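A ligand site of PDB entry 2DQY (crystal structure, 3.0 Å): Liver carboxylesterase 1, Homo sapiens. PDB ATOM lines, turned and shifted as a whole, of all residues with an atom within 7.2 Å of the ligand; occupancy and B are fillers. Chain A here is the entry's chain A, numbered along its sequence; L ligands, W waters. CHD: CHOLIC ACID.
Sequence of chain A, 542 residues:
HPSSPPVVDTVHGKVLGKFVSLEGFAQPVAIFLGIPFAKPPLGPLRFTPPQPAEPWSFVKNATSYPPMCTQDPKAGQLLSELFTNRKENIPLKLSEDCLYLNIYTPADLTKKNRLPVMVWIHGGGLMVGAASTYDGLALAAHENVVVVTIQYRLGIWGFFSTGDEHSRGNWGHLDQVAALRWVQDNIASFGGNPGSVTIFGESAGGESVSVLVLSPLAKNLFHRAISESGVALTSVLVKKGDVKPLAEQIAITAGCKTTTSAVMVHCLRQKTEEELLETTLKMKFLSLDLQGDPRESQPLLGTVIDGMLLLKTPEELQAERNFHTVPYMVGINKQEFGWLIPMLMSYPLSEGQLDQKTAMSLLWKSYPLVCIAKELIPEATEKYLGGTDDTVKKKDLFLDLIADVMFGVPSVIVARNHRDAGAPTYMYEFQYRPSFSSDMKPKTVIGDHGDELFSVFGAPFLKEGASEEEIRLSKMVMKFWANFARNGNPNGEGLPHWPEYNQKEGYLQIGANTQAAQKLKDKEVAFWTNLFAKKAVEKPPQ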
ATOM      1  N   PHE A 337     -21.812   4.856 -22.082  1.00  0.00           N
ATOM      2  CA  PHE A 337     -22.631   3.692 -21.796  1.00  0.00           C
ATOM      3  C   PHE A 337     -21.734   2.588 -21.260  1.00  0.00           C
ATOM      4  O   PHE A 337     -21.995   1.404 -21.482  1.00  0.00           O
ATOM      5  CB  PHE A 337     -23.347   3.235 -23.078  1.00  0.00           C
ATOM      6  CG  PHE A 337     -24.658   2.553 -22.822  1.00  0.00           C
ATOM      7  CD1 PHE A 337     -24.848   1.241 -23.230  1.00  0.00           C
ATOM      8  CD2 PHE A 337     -25.681   3.207 -22.153  1.00  0.00           C
ATOM      9  CE1 PHE A 337     -26.043   0.595 -22.975  1.00  0.00           C
ATOM     10  CE2 PHE A 337     -26.878   2.577 -21.892  1.00  0.00           C
ATOM     11  CZ  PHE A 337     -27.052   1.262 -22.304  1.00  0.00           C
ATOM     12  N   GLY A 338     -20.700   2.989 -20.537  1.00  0.00           N
ATOM     13  CA  GLY A 338     -19.763   2.036 -19.977  1.00  0.00           C
ATOM     14  C   GLY A 338     -20.270   1.014 -18.970  1.00  0.00           C
ATOM     15  O   GLY A 338     -20.113  -0.185 -19.146  1.00  0.00           O
ATOM     16  N   TRP A 339     -20.878   1.500 -17.890  1.00  0.00           N
ATOM     17  CA  TRP A 339     -21.372   0.601 -16.873  1.00  0.00           C
ATOM     18  C   TRP A 339     -22.625   1.115 -16.176  1.00  0.00           C
ATOM     19  O   TRP A 339     -23.655   0.421 -16.125  1.00  0.00           O
ATOM     20  CB  TRP A 339     -20.264   0.353 -15.836  1.00  0.00           C
ATOM     21  CG  TRP A 339     -20.729  -0.414 -14.623  1.00  0.00           C
ATOM     22  CD1 TRP A 339     -20.963  -1.760 -14.543  1.00  0.00           C
ATOM     23  CD2 TRP A 339     -21.091   0.124 -13.353  1.00  0.00           C
ATOM     24  NE1 TRP A 339     -21.461  -2.092 -13.305  1.00  0.00           N
ATOM     25  CE2 TRP A 339     -21.550  -0.947 -12.557  1.00  0.00           C
ATOM     26  CE3 TRP A 339     -21.092   1.417 -12.811  1.00  0.00           C
ATOM     27  CZ2 TRP A 339     -22.011  -0.765 -11.244  1.00  0.00           C
ATOM     28  CZ3 TRP A 339     -21.551   1.583 -11.505  1.00  0.00           C
ATOM     29  CH2 TRP A 339     -22.001   0.506 -10.737  1.00  0.00           C
ATOM     30  N   LEU A 340     -22.536   2.338 -15.643  1.00  0.00           N
ATOM     31  CA  LEU A 340     -23.621   2.990 -14.908  1.00  0.00           C
ATOM     32  C   LEU A 340     -25.016   2.849 -15.517  1.00  0.00           C
ATOM     33  O   LEU A 340     -25.875   2.173 -14.940  1.00  0.00           O
ATOM     34  CB  LEU A 340     -23.305   4.472 -14.721  1.00  0.00           C
ATOM     35  CG  LEU A 340     -24.308   5.218 -13.839  1.00  0.00           C
ATOM     36  CD1 LEU A 340     -24.247   4.672 -12.432  1.00  0.00           C
ATOM     37  CD2 LEU A 340     -23.978   6.705 -13.863  1.00  0.00           C
ATOM     38  N   PRO A 342     -26.175   1.145 -18.274  1.00  0.00           N
ATOM     39  CA  PRO A 342     -26.502  -0.266 -18.523  1.00  0.00           C
ATOM     40  C   PRO A 342     -26.782  -1.086 -17.269  1.00  0.00           C
ATOM     41  O   PRO A 342     -27.636  -1.961 -17.260  1.00  0.00           O
ATOM     42  CB  PRO A 342     -25.272  -0.797 -19.246  1.00  0.00           C
ATOM     43  CG  PRO A 342     -24.811   0.370 -19.987  1.00  0.00           C
ATOM     44  CD  PRO A 342     -24.936   1.497 -18.989  1.00  0.00           C
ATOM     45  N   MET A 343     -26.047  -0.798 -16.202  1.00  0.00           N
ATOM     46  CA  MET A 343     -26.227  -1.516 -14.958  1.00  0.00           C
ATOM     47  C   MET A 343     -27.585  -1.205 -14.338  1.00  0.00           C
ATOM     48  O   MET A 343     -28.176  -2.067 -13.685  1.00  0.00           O
ATOM     49  CB  MET A 343     -25.098  -1.163 -13.978  1.00  0.00           C
ATOM     50  CG  MET A 343     -25.235  -1.727 -12.569  1.00  0.00           C
ATOM     51  SD  MET A 343     -26.312  -0.780 -11.453  1.00  0.00           S
ATOM     52  CE  MET A 343     -25.231   0.571 -10.928  1.00  0.00           C
ATOM     53  N   TYR A 347     -29.451  -4.154 -18.335  1.00  0.00           N
ATOM     54  CA  TYR A 347     -29.112  -4.670 -19.661  1.00  0.00           C
ATOM     55  C   TYR A 347     -28.547  -6.090 -19.609  1.00  0.00           C
ATOM     56  O   TYR A 347     -27.671  -6.399 -18.798  1.00  0.00           O
ATOM     57  CB  TYR A 347     -28.103  -3.764 -20.345  1.00  0.00           C
ATOM     58  CG  TYR A 347     -28.722  -2.878 -21.398  1.00  0.00           C
ATOM     59  CD1 TYR A 347     -29.741  -2.000 -21.066  1.00  0.00           C
ATOM     60  CD2 TYR A 347     -28.280  -2.913 -22.716  1.00  0.00           C
ATOM     61  CE1 TYR A 347     -30.312  -1.188 -22.011  1.00  0.00           C
ATOM     62  CE2 TYR A 347     -28.845  -2.106 -23.680  1.00  0.00           C
ATOM     63  CZ  TYR A 347     -29.866  -1.245 -23.324  1.00  0.00           C
ATOM     64  OH  TYR A 347     -30.448  -0.408 -24.257  1.00  0.00           O
ATOM     65  N   PRO A 348     -29.055  -6.966 -20.486  1.00  0.00           N
ATOM     66  CA  PRO A 348     -28.662  -8.369 -20.625  1.00  0.00           C
ATOM     67  C   PRO A 348     -27.220  -8.631 -21.108  1.00  0.00           C
ATOM     68  O   PRO A 348     -26.972  -9.573 -21.867  1.00  0.00           O
ATOM     69  CB  PRO A 348     -29.694  -8.910 -21.618  1.00  0.00           C
ATOM     70  CG  PRO A 348     -30.899  -8.092 -21.303  1.00  0.00           C
ATOM     71  CD  PRO A 348     -30.303  -6.703 -21.206  1.00  0.00           C
ATOM     72  N   LEU A 349     -26.279  -7.812 -20.667  1.00  0.00           N
ATOM     73  CA  LEU A 349     -24.886  -7.987 -21.056  1.00  0.00           C
ATOM     74  C   LEU A 349     -24.112  -8.814 -20.051  1.00  0.00           C
ATOM     75  O   LEU A 349     -22.903  -9.004 -20.197  1.00  0.00           O
ATOM     76  CB  LEU A 349     -24.193  -6.650 -21.228  1.00  0.00           C
ATOM     77  CG  LEU A 349     -24.564  -5.905 -22.502  1.00  0.00           C
ATOM     78  CD1 LEU A 349     -23.738  -4.638 -22.528  1.00  0.00           C
ATOM     79  CD2 LEU A 349     -24.298  -6.766 -23.746  1.00  0.00           C
ATOM     80  N   SER A 350     -24.799  -9.290 -19.028  1.00  0.00           N
ATOM     81  CA  SER A 350     -24.197 -10.095 -17.976  1.00  0.00           C
ATOM     82  C   SER A 350     -23.316 -11.245 -18.479  1.00  0.00           C
ATOM     83  O   SER A 350     -22.426 -11.709 -17.760  1.00  0.00           O
ATOM     84  CB  SER A 350     -25.289 -10.638 -17.053  1.00  0.00           C
ATOM     85  OG  SER A 350     -26.350 -11.201 -17.815  1.00  0.00           O
ATOM     86  N   GLU A 351     -23.568 -11.708 -19.713  1.00  0.00           N
ATOM     87  CA  GLU A 351     -22.770 -12.795 -20.290  1.00  0.00           C
ATOM     88  C   GLU A 351     -21.284 -12.457 -20.359  1.00  0.00           C
ATOM     89  O   GLU A 351     -20.426 -13.313 -20.094  1.00  0.00           O
ATOM     90  CB  GLU A 351     -23.278 -13.147 -21.697  1.00  0.00           C
ATOM     91  CG  GLU A 351     -24.374 -14.215 -21.718  1.00  0.00           C
ATOM     92  CD  GLU A 351     -23.881 -15.566 -21.231  1.00  0.00           C
ATOM     93  OE1 GLU A 351     -22.959 -16.123 -21.869  1.00  0.00           O
ATOM     94  OE2 GLU A 351     -24.410 -16.070 -20.214  1.00  0.00           O
ATOM     95  N   GLY A 352     -20.964 -11.211 -20.702  1.00  0.00           N
ATOM     96  CA  GLY A 352     -19.581 -10.782 -20.782  1.00  0.00           C
ATOM     97  C   GLY A 352     -19.159 -10.441 -22.188  1.00  0.00           C
ATOM     98  O   GLY A 352     -18.234  -9.644 -22.393  1.00  0.00           O
ATOM     99  N   GLN A 353     -19.826 -11.053 -23.163  1.00  0.00           N
ATOM    100  CA  GLN A 353     -19.533 -10.825 -24.566  1.00  0.00           C
ATOM    101  C   GLN A 353     -20.829 -10.708 -25.369  1.00  0.00           C
ATOM    102  O   GLN A 353     -21.922 -10.831 -24.815  1.00  0.00           O
ATOM    103  CB  GLN A 353     -18.688 -11.968 -25.136  1.00  0.00           C
ATOM    104  CG  GLN A 353     -19.372 -13.334 -25.127  1.00  0.00           C
ATOM    105  CD  GLN A 353     -19.449 -13.962 -23.749  1.00  0.00           C
ATOM    106  OE1 GLN A 353     -18.437 -14.414 -23.207  1.00  0.00           O
ATOM    107  NE2 GLN A 353     -20.642 -13.989 -23.174  1.00  0.00           N
ATOM    108  N   LYS A 395     -19.036  -6.609 -27.559  1.00  0.00           N
ATOM    109  CA  LYS A 395     -19.808  -6.062 -26.450  1.00  0.00           C
ATOM    110  C   LYS A 395     -19.367  -4.624 -26.222  1.00  0.00           C
ATOM    111  O   LYS A 395     -20.184  -3.714 -26.098  1.00  0.00           O
ATOM    112  CB  LYS A 395     -19.549  -6.848 -25.162  1.00  0.00           C
ATOM    113  CG  LYS A 395     -20.302  -6.309 -23.958  1.00  0.00           C
ATOM    114  CD  LYS A 395     -19.817  -6.901 -22.637  1.00  0.00           C
ATOM    115  CE  LYS A 395     -18.413  -6.416 -22.292  1.00  0.00           C
ATOM    116  NZ  LYS A 395     -17.948  -6.997 -21.001  1.00  0.00           N
ATOM    117  N   ASP A 396     -18.057  -4.459 -26.163  1.00  0.00           N
ATOM    118  CA  ASP A 396     -17.443  -3.175 -25.942  1.00  0.00           C
ATOM    119  C   ASP A 396     -17.780  -2.204 -27.058  1.00  0.00           C
ATOM    120  O   ASP A 396     -18.175  -1.064 -26.810  1.00  0.00           O
ATOM    121  CB  ASP A 396     -15.932  -3.362 -25.815  1.00  0.00           C
ATOM    122  CG  ASP A 396     -15.553  -4.045 -24.510  1.00  0.00           C
ATOM    123  OD1 ASP A 396     -16.411  -4.740 -23.917  1.00  0.00           O
ATOM    124  OD2 ASP A 396     -14.389  -3.898 -24.076  1.00  0.00           O
ATOM    125  N   LEU A 399     -21.344  -1.182 -26.801  1.00  0.00           N
ATOM    126  CA  LEU A 399     -21.563  -0.164 -25.790  1.00  0.00           C
ATOM    127  C   LEU A 399     -21.155   1.201 -26.343  1.00  0.00           C
ATOM    128  O   LEU A 399     -21.682   2.233 -25.933  1.00  0.00           O
ATOM    129  CB  LEU A 399     -20.755  -0.474 -24.528  1.00  0.00           C
ATOM    130  CG  LEU A 399     -21.183  -1.706 -23.720  1.00  0.00           C
ATOM    131  CD1 LEU A 399     -20.195  -1.969 -22.601  1.00  0.00           C
ATOM    132  CD2 LEU A 399     -22.571  -1.492 -23.143  1.00  0.00           C
ATOM    133  N   ASP A 439     -17.781  -0.579  -6.597  1.00  0.00           N
ATOM    134  CA  ASP A 439     -16.973  -1.774  -6.534  1.00  0.00           C
ATOM    135  C   ASP A 439     -17.401  -2.734  -7.634  1.00  0.00           C
ATOM    136  O   ASP A 439     -16.601  -3.535  -8.099  1.00  0.00           O
ATOM    137  CB  ASP A 439     -17.146  -2.440  -5.191  1.00  0.00           C
ATOM    138  CG  ASP A 439     -16.680  -1.559  -4.061  1.00  0.00           C
ATOM    139  OD1 ASP A 439     -15.456  -1.495  -3.816  1.00  0.00           O
ATOM    140  OD2 ASP A 439     -17.546  -0.910  -3.435  1.00  0.00           O
ATOM    141  N   MET A 440     -18.656  -2.641  -8.042  1.00  0.00           N
ATOM    142  CA  MET A 440     -19.164  -3.536  -9.075  1.00  0.00           C
ATOM    143  C   MET A 440     -18.856  -2.974 -10.458  1.00  0.00           C
ATOM    144  O   MET A 440     -19.356  -3.483 -11.464  1.00  0.00           O
ATOM    145  CB  MET A 440     -20.667  -3.734  -8.912  1.00  0.00           C
ATOM    146  CG  MET A 440     -21.101  -4.120  -7.522  1.00  0.00           C
ATOM    147  SD  MET A 440     -22.895  -4.314  -7.467  1.00  0.00           S
ATOM    148  CE  MET A 440     -23.501  -2.515  -7.656  1.00  0.00           C
ATOM    149  N   LYS A 441     -18.020  -1.949 -10.494  1.00  0.00           N
ATOM    150  CA  LYS A 441     -17.634  -1.331 -11.745  1.00  0.00           C
ATOM    151  C   LYS A 441     -16.295  -1.876 -12.224  1.00  0.00           C
ATOM    152  O   LYS A 441     -15.299  -1.783 -11.513  1.00  0.00           O
ATOM    153  CB  LYS A 441     -17.539   0.189 -11.543  1.00  0.00           C
ATOM    154  CG  LYS A 441     -17.082   0.920 -12.762  1.00  0.00           C
ATOM    155  CD  LYS A 441     -16.740   2.348 -12.447  1.00  0.00           C
ATOM    156  CE  LYS A 441     -16.265   3.064 -13.700  1.00  0.00           C
ATOM    157  NZ  LYS A 441     -16.177   4.528 -13.488  1.00  0.00           N
ATOM    158  N   PRO A 442     -16.244  -2.465 -13.426  1.00  0.00           N
ATOM    159  CA  PRO A 442     -14.981  -3.007 -13.943  1.00  0.00           C
ATOM    160  C   PRO A 442     -13.849  -1.981 -14.009  1.00  0.00           C
ATOM    161  O   PRO A 442     -14.068  -0.820 -14.351  1.00  0.00           O
ATOM    162  CB  PRO A 442     -15.377  -3.538 -15.339  1.00  0.00           C
ATOM    163  CG  PRO A 442     -16.594  -2.740 -15.701  1.00  0.00           C
ATOM    164  CD  PRO A 442     -17.344  -2.669 -14.397  1.00  0.00           C
ATOM    165  N   LYS A 443     -12.632  -2.402 -13.684  1.00  0.00           N
ATOM    166  CA  LYS A 443     -11.539  -1.448 -13.694  1.00  0.00           C
ATOM    167  C   LYS A 443     -11.004  -1.166 -15.071  1.00  0.00           C
ATOM    168  O   LYS A 443      -9.961  -0.532 -15.212  1.00  0.00           O
ATOM    169  CB  LYS A 443     -10.416  -1.923 -12.786  1.00  0.00           C
ATOM    170  CG  LYS A 443     -10.850  -2.149 -11.345  1.00  0.00           C
ATOM    171  CD  LYS A 443      -9.658  -2.181 -10.422  1.00  0.00           C
ATOM    172  CE  LYS A 443     -10.066  -2.360  -8.982  1.00  0.00           C
ATOM    173  NZ  LYS A 443      -8.867  -2.226  -8.093  1.00  0.00           N
ATOM    174  N   THR A 444     -11.725  -1.614 -16.098  1.00  0.00           N
ATOM    175  CA  THR A 444     -11.299  -1.375 -17.470  1.00  0.00           C
ATOM    176  C   THR A 444     -12.126  -0.245 -18.096  1.00  0.00           C
ATOM    177  O   THR A 444     -11.848   0.214 -19.220  1.00  0.00           O
ATOM    178  CB  THR A 444     -11.445  -2.657 -18.343  1.00  0.00           C
ATOM    179  OG1 THR A 444     -12.831  -2.917 -18.590  1.00  0.00           O
ATOM    180  CG2 THR A 444     -10.838  -3.854 -17.637  1.00  0.00           C
ATOM    181  N   VAL A 445     -13.136   0.225 -17.351  1.00  0.00           N
ATOM    182  CA  VAL A 445     -14.029   1.308 -17.795  1.00  0.00           C
ATOM    183  C   VAL A 445     -13.600   2.705 -17.347  1.00  0.00           C
ATOM    184  O   VAL A 445     -13.730   3.086 -16.192  1.00  0.00           O
ATOM    185  CB  VAL A 445     -15.487   1.066 -17.316  1.00  0.00           C
ATOM    186  CG1 VAL A 445     -16.330   2.305 -17.573  1.00  0.00           C
ATOM    187  CG2 VAL A 445     -16.095  -0.124 -18.030  1.00  0.00           C
HETATM  188  C1  CHD L   1     -22.397  -4.834 -17.067  1.00  0.00           C
HETATM  189  C2  CHD L   1     -21.305  -3.800 -17.535  1.00  0.00           C
HETATM  190  C3  CHD L   1     -20.792  -4.209 -18.955  1.00  0.00           C
HETATM  191  O3  CHD L   1     -19.788  -3.292 -19.406  1.00  0.00           O
HETATM  192  C4  CHD L   1     -20.198  -5.644 -18.923  1.00  0.00           C
HETATM  193  C5  CHD L   1     -21.270  -6.683 -18.382  1.00  0.00           C
HETATM  194  C6  CHD L   1     -20.646  -8.140 -18.335  1.00  0.00           C
HETATM  195  C7  CHD L   1     -19.549  -8.292 -17.247  1.00  0.00           C
HETATM  196  O7  CHD L   1     -18.389  -7.527 -17.593  1.00  0.00           O
HETATM  197  C8  CHD L   1     -20.107  -7.892 -15.830  1.00  0.00           C
HETATM  198  C9  CHD L   1     -20.668  -6.404 -15.862  1.00  0.00           C
HETATM  199  C10 CHD L   1     -21.827  -6.272 -16.945  1.00  0.00           C
HETATM  200  C11 CHD L   1     -21.158  -6.027 -14.407  1.00  0.00           C
HETATM  201  C12 CHD L   1     -19.959  -6.135 -13.369  1.00  0.00           C
HETATM  202  O12 CHD L   1     -18.908  -5.250 -13.852  1.00  0.00           O
HETATM  203  C13 CHD L   1     -19.409  -7.605 -13.280  1.00  0.00           C
HETATM  204  C14 CHD L   1     -18.972  -7.978 -14.754  1.00  0.00           C
HETATM  205  C15 CHD L   1     -18.282  -9.348 -14.575  1.00  0.00           C
HETATM  206  C16 CHD L   1     -17.379  -9.054 -13.346  1.00  0.00           C
HETATM  207  C17 CHD L   1     -17.987  -7.816 -12.598  1.00  0.00           C
HETATM  208  C18 CHD L   1     -20.525  -8.583 -12.713  1.00  0.00           C
HETATM  209  C19 CHD L   1     -23.073  -7.133 -16.544  1.00  0.00           C
HETATM  210  C20 CHD L   1     -17.899  -8.085 -11.026  1.00  0.00           C
HETATM  211  C21 CHD L   1     -18.500  -6.918 -10.185  1.00  0.00           C
HETATM  212  C22 CHD L   1     -16.396  -8.229 -10.654  1.00  0.00           C
HETATM  213  C23 CHD L   1     -16.135  -9.185  -9.469  1.00  0.00           C
HETATM  214  O25 CHD L   1     -14.653  -9.265  -7.472  1.00  0.00           O
HETATM  215  C24 CHD L   1     -15.049  -8.585  -8.556  1.00  0.00           C
HETATM  216  O26 CHD L   1     -14.556  -7.511  -8.804  1.00  0.00           O
HETATM  217  O   HOH W   1     -14.200 -11.613  -8.862  1.00  0.00           O
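O of Met 440 lies within hydrogen-bond range of O12 of the ligand, 3.0 Å away.
An oxygen (O3) of the ligand is in hydrogen-bond range of the backbone carbonyl oxygen (O) of Gly 338 (3.1 Å).
O7 of the ligand lies close to NZ of Lys 395, at 3.5 Å.
The side-chain amino group (NZ) of Lys 395 is in salt-bridge range of the side-chain carboxylate (OD1) of Asp 396 (3.99 Å).
The indole nitrogen (NE1) of Trp 339 sits at hydrogen-bond distance from the backbone carbonyl oxygen (O) of Met 440 (3.1 Å).
NZ of Lys 395 lies within hydrogen-bond range of O of Gly 352, at 3.0 Å.
Merely in contact with the ligand: Leu 349, Pro 442, Ser 350, Leu 399, Trp 339 and Gly 352.
Nine residues have an atom within 4 Å of the ligand: Gly 338, Trp 339, Leu 349, Ser 350, Gly 352, Lys 395, Leu 399, Met 440 and Pro 442.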
